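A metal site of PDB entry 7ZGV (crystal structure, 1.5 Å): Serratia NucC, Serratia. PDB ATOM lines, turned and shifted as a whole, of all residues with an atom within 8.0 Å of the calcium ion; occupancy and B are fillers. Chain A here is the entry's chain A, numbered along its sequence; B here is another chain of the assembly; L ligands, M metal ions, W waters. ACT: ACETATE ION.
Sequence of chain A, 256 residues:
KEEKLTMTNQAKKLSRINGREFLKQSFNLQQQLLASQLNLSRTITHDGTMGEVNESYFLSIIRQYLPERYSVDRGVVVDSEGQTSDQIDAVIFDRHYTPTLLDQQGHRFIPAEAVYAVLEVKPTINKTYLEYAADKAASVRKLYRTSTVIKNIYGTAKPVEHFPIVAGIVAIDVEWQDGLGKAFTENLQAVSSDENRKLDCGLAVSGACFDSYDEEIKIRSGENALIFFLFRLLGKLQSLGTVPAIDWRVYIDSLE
Along chain A the residues within 4 Å of the calcium ion span positions 52 to 121.
The calcium ion is bound by O of Val 121 (2.3 Å), OD2 of Asp 89 (2.4 Å), water W1 (2.4 Å), OE2 of Glu 52 of chain A (2.5 Å), O of the ligand (2.5 Å), OXT of the ligand (2.5 Å) and OE2 of Glu 120 (2.6 Å).
N of Val 170 lies within hydrogen-bond range of O of Glu 120, 2.8 Å away.
OE2 of Glu 120 lies close to NZ of Lys 122, at 3.5 Å.
The side-chain amino group (NZ) of Lys 136 lies within salt-bridge range of the side-chain carboxylate (OE1) of Glu 120 (2.7 Å).
The side-chain carboxylate (OE1) of Glu 52 of chain A sits at hydrogen-bond distance from the backbone NH (N) of Glu 52 of chain B (3.4 Å).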
ATOM      1  N   GLY A  48     -14.191   8.129  29.577  1.00  0.00           N
ATOM      2  CA  GLY A  48     -15.169   9.174  29.742  1.00  0.00           C
ATOM      3  C   GLY A  48     -15.892   9.188  31.076  1.00  0.00           C
ATOM      4  O   GLY A  48     -16.842   9.961  31.254  1.00  0.00           O
ATOM      5  N   GLY A  51     -14.150  12.355  33.487  1.00  0.00           N
ATOM      6  CA  GLY A  51     -13.870  13.525  32.693  1.00  0.00           C
ATOM      7  C   GLY A  51     -14.271  13.287  31.252  1.00  0.00           C
ATOM      8  O   GLY A  51     -14.409  12.145  30.836  1.00  0.00           O
ATOM      9  N   GLU A  52     -14.485  14.362  30.485  1.00  0.00           N
ATOM     10  CA  GLU A  52     -14.846  14.196  29.089  1.00  0.00           C
ATOM     11  C   GLU A  52     -13.584  13.982  28.262  1.00  0.00           C
ATOM     12  O   GLU A  52     -12.513  14.475  28.600  1.00  0.00           O
ATOM     13  CB  GLU A  52     -15.600  15.389  28.518  1.00  0.00           C
ATOM     14  CG  GLU A  52     -17.115  15.157  28.410  1.00  0.00           C
ATOM     15  CD  GLU A  52     -17.847  16.216  27.569  1.00  0.00           C
ATOM     16  OE1 GLU A  52     -18.081  17.300  28.186  1.00  0.00           O
ATOM     17  OE2 GLU A  52     -18.190  15.954  26.348  1.00  0.00           O
ATOM     18  N   VAL A  53     -13.711  13.179  27.204  1.00  0.00           N
ATOM     19  CA  VAL A  53     -12.621  13.058  26.251  1.00  0.00           C
ATOM     20  C   VAL A  53     -12.317  14.460  25.739  1.00  0.00           C
ATOM     21  O   VAL A  53     -13.232  15.226  25.386  1.00  0.00           O
ATOM     22  CB  VAL A  53     -13.041  12.131  25.098  1.00  0.00           C
ATOM     23  CG1 VAL A  53     -11.974  12.058  24.043  1.00  0.00           C
ATOM     24  CG2 VAL A  53     -13.350  10.715  25.641  1.00  0.00           C
ATOM     25  N   ASN A  54     -11.025  14.808  25.674  1.00  0.00           N
ATOM     26  CA  ASN A  54     -10.626  16.177  25.319  1.00  0.00           C
ATOM     27  C   ASN A  54     -10.744  16.401  23.820  1.00  0.00           C
ATOM     28  O   ASN A  54      -9.936  15.892  23.049  1.00  0.00           O
ATOM     29  CB  ASN A  54      -9.228  16.456  25.856  1.00  0.00           C
ATOM     30  CG  ASN A  54      -8.818  17.886  25.684  1.00  0.00           C
ATOM     31  OD1 ASN A  54      -9.384  18.562  24.848  1.00  0.00           O
ATOM     32  ND2 ASN A  54      -7.948  18.369  26.504  1.00  0.00           N
ATOM     33  N   GLU A  55     -11.779  17.130  23.416  1.00  0.00           N
ATOM     34  CA  GLU A  55     -12.062  17.425  22.018  1.00  0.00           C
ATOM     35  C   GLU A  55     -11.133  18.481  21.407  1.00  0.00           C
ATOM     36  O   GLU A  55     -11.215  18.696  20.190  1.00  0.00           O
ATOM     37  CB  GLU A  55     -13.498  17.941  21.842  1.00  0.00           C
ATOM     38  CG  GLU A  55     -13.805  19.272  22.543  1.00  0.00           C
ATOM     39  CD  GLU A  55     -13.858  19.139  24.082  1.00  0.00           C
ATOM     40  OE1 GLU A  55     -14.391  18.136  24.607  1.00  0.00           O
ATOM     41  OE2 GLU A  55     -13.392  20.058  24.763  1.00  0.00           O
ATOM     42  N   GLN A  87     -24.640  20.898  25.837  1.00  0.00           N
ATOM     43  CA  GLN A  87     -23.259  21.293  25.549  1.00  0.00           C
ATOM     44  C   GLN A  87     -22.746  20.460  24.380  1.00  0.00           C
ATOM     45  O   GLN A  87     -22.915  19.242  24.379  1.00  0.00           O
ATOM     46  CB  GLN A  87     -22.334  21.121  26.765  1.00  0.00           C
ATOM     47  CG  GLN A  87     -22.570  22.149  27.880  1.00  0.00           C
ATOM     48  CD  GLN A  87     -21.313  22.621  28.662  1.00  0.00           C
ATOM     49  OE1 GLN A  87     -21.238  23.844  29.056  1.00  0.00           O
ATOM     50  NE2 GLN A  87     -20.342  21.674  28.932  1.00  0.00           N
ATOM     51  N   ILE A  88     -22.177  21.124  23.376  1.00  0.00           N
ATOM     52  CA  ILE A  88     -21.796  20.487  22.114  1.00  0.00           C
ATOM     53  C   ILE A  88     -20.275  20.514  22.007  1.00  0.00           C
ATOM     54  O   ILE A  88     -19.636  21.534  22.277  1.00  0.00           O
ATOM     55  CB  ILE A  88     -22.426  21.201  20.897  1.00  0.00           C
ATOM     56  CG1 ILE A  88     -23.958  21.312  21.014  1.00  0.00           C
ATOM     57  CG2 ILE A  88     -22.014  20.488  19.591  1.00  0.00           C
ATOM     58  CD1 ILE A  88     -24.663  20.004  21.205  1.00  0.00           C
ATOM     59  N   ASP A  89     -19.681  19.373  21.641  1.00  0.00           N
ATOM     60  CA  ASP A  89     -18.232  19.266  21.629  1.00  0.00           C
ATOM     61  C   ASP A  89     -17.611  20.014  20.453  1.00  0.00           C
ATOM     62  O   ASP A  89     -16.543  20.593  20.575  1.00  0.00           O
ATOM     63  CB  ASP A  89     -17.811  17.793  21.536  1.00  0.00           C
ATOM     64  CG  ASP A  89     -18.064  17.034  22.818  1.00  0.00           C
ATOM     65  OD1 ASP A  89     -18.310  17.652  23.884  1.00  0.00           O
ATOM     66  OD2 ASP A  89     -18.057  15.782  22.760  1.00  0.00           O
ATOM     67  N   ALA A  90     -18.264  19.998  19.294  1.00  0.00           N
ATOM     68  CA  ALA A  90     -17.708  20.669  18.138  1.00  0.00           C
ATOM     69  C   ALA A  90     -18.851  21.184  17.282  1.00  0.00           C
ATOM     70  O   ALA A  90     -19.701  20.419  16.815  1.00  0.00           O
ATOM     71  CB  ALA A  90     -16.842  19.724  17.308  1.00  0.00           C
ATOM     72  N   LEU A 119     -20.746  17.918  16.022  1.00  0.00           N
ATOM     73  CA  LEU A 119     -20.149  16.607  16.217  1.00  0.00           C
ATOM     74  C   LEU A 119     -19.907  16.388  17.709  1.00  0.00           C
ATOM     75  O   LEU A 119     -19.519  17.318  18.424  1.00  0.00           O
ATOM     76  CB  LEU A 119     -18.819  16.506  15.464  1.00  0.00           C
ATOM     77  CG  LEU A 119     -18.773  16.801  13.961  1.00  0.00           C
ATOM     78  CD1 LEU A 119     -17.310  17.128  13.499  1.00  0.00           C
ATOM     79  CD2 LEU A 119     -19.228  15.615  13.184  1.00  0.00           C
ATOM     80  N   GLU A 120     -20.155  15.166  18.183  1.00  0.00           N
ATOM     81  CA  GLU A 120     -19.912  14.770  19.548  1.00  0.00           C
ATOM     82  C   GLU A 120     -18.734  13.834  19.581  1.00  0.00           C
ATOM     83  O   GLU A 120     -18.667  12.892  18.766  1.00  0.00           O
ATOM     84  CB  GLU A 120     -21.143  14.088  20.133  1.00  0.00           C
ATOM     85  CG  GLU A 120     -20.897  13.309  21.437  1.00  0.00           C
ATOM     86  CD  GLU A 120     -20.780  14.180  22.698  1.00  0.00           C
ATOM     87  OE1 GLU A 120     -21.364  15.305  22.751  1.00  0.00           O
ATOM     88  OE2 GLU A 120     -20.135  13.690  23.681  1.00  0.00           O
ATOM     89  N   VAL A 121     -17.822  14.074  20.538  1.00  0.00           N
ATOM     90  CA  VAL A 121     -16.615  13.250  20.709  1.00  0.00           C
ATOM     91  C   VAL A 121     -16.866  12.282  21.863  1.00  0.00           C
ATOM     92  O   VAL A 121     -17.183  12.687  22.995  1.00  0.00           O
ATOM     93  CB  VAL A 121     -15.377  14.121  20.975  1.00  0.00           C
ATOM     94  CG1 VAL A 121     -14.187  13.222  21.231  1.00  0.00           C
ATOM     95  CG2 VAL A 121     -15.088  15.062  19.826  1.00  0.00           C
ATOM     96  N   LYS A 122     -16.729  10.986  21.585  1.00  0.00           N
ATOM     97  CA  LYS A 122     -17.011   9.916  22.534  1.00  0.00           C
ATOM     98  C   LYS A 122     -15.885   8.893  22.546  1.00  0.00           C
ATOM     99  O   LYS A 122     -15.010   8.870  21.674  1.00  0.00           O
ATOM    100  CB  LYS A 122     -18.339   9.203  22.189  1.00  0.00           C
ATOM    101  CG  LYS A 122     -19.559  10.005  22.582  1.00  0.00           C
ATOM    102  CD  LYS A 122     -19.633  10.072  24.114  1.00  0.00           C
ATOM    103  CE  LYS A 122     -20.914  10.637  24.562  1.00  0.00           C
ATOM    104  NZ  LYS A 122     -20.757  11.062  25.975  1.00  0.00           N
ATOM    105  N   PRO A 123     -15.861   8.011  23.550  1.00  0.00           N
ATOM    106  CA  PRO A 123     -14.771   7.038  23.625  1.00  0.00           C
ATOM    107  C   PRO A 123     -14.727   6.087  22.444  1.00  0.00           C
ATOM    108  O   PRO A 123     -13.638   5.726  22.001  1.00  0.00           O
ATOM    109  CB  PRO A 123     -15.061   6.326  24.956  1.00  0.00           C
ATOM    110  CG  PRO A 123     -15.792   7.337  25.783  1.00  0.00           C
ATOM    111  CD  PRO A 123     -16.680   8.026  24.783  1.00  0.00           C
ATOM    112  N   LYS A 136     -27.488  14.644  21.293  1.00  0.00           N
ATOM    113  CA  LYS A 136     -26.884  15.968  21.199  1.00  0.00           C
ATOM    114  C   LYS A 136     -27.329  16.655  19.917  1.00  0.00           C
ATOM    115  O   LYS A 136     -27.675  17.850  19.924  1.00  0.00           O
ATOM    116  CB  LYS A 136     -25.343  15.860  21.225  1.00  0.00           C
ATOM    117  CG  LYS A 136     -24.685  15.480  22.555  1.00  0.00           C
ATOM    118  CD  LYS A 136     -24.921  16.547  23.656  1.00  0.00           C
ATOM    119  CE  LYS A 136     -24.027  16.334  24.901  1.00  0.00           C
ATOM    120  NZ  LYS A 136     -22.586  16.644  24.722  1.00  0.00           N
ATOM    121  N   VAL A 170     -17.399  11.523  16.614  1.00  0.00           N
ATOM    122  CA  VAL A 170     -15.966  11.309  16.506  1.00  0.00           C
ATOM    123  C   VAL A 170     -15.561  10.469  17.701  1.00  0.00           C
ATOM    124  O   VAL A 170     -15.988  10.749  18.825  1.00  0.00           O
ATOM    125  CB  VAL A 170     -15.212  12.646  16.476  1.00  0.00           C
ATOM    126  CG1 VAL A 170     -13.684  12.414  16.431  1.00  0.00           C
ATOM    127  CG2 VAL A 170     -15.701  13.414  15.251  1.00  0.00           C
ATOM    128  N   GLY B  51     -21.962  16.304  30.993  1.00  0.00           N
ATOM    129  CA  GLY B  51     -20.849  17.063  30.480  1.00  0.00           C
ATOM    130  C   GLY B  51     -20.120  17.752  31.614  1.00  0.00           C
ATOM    131  O   GLY B  51     -20.687  17.927  32.691  1.00  0.00           O
ATOM    132  N   GLU B  52     -18.867  18.131  31.392  1.00  0.00           N
ATOM    133  CA  GLU B  52     -18.126  18.824  32.446  1.00  0.00           C
ATOM    134  C   GLU B  52     -18.467  20.310  32.409  1.00  0.00           C
ATOM    135  O   GLU B  52     -18.786  20.871  31.366  1.00  0.00           O
ATOM    136  CB  GLU B  52     -16.607  18.679  32.298  1.00  0.00           C
ATOM    137  CG  GLU B  52     -16.013  17.640  33.271  1.00  0.00           C
ATOM    138  CD  GLU B  52     -14.473  17.697  33.354  1.00  0.00           C
ATOM    139  OE1 GLU B  52     -13.877  17.124  32.398  1.00  0.00           O
ATOM    140  OE2 GLU B  52     -13.902  18.281  34.361  1.00  0.00           O
HETATM  141  C   ACT L   1     -17.338  12.376  26.518  1.00  0.00           C
HETATM  142  O   ACT L   1     -18.556  12.616  26.242  1.00  0.00           O
HETATM  143  OXT ACT L   1     -16.300  12.998  26.143  1.00  0.00           O
HETATM  144  CH3 ACT L   1     -17.109  11.201  27.490  1.00  0.00           C
HETATM  145 CA    CA M   1     -17.759  14.281  24.603  1.00  0.00          CA
HETATM  146  O   HOH W   1     -15.681  15.481  24.486  1.00  0.00           O
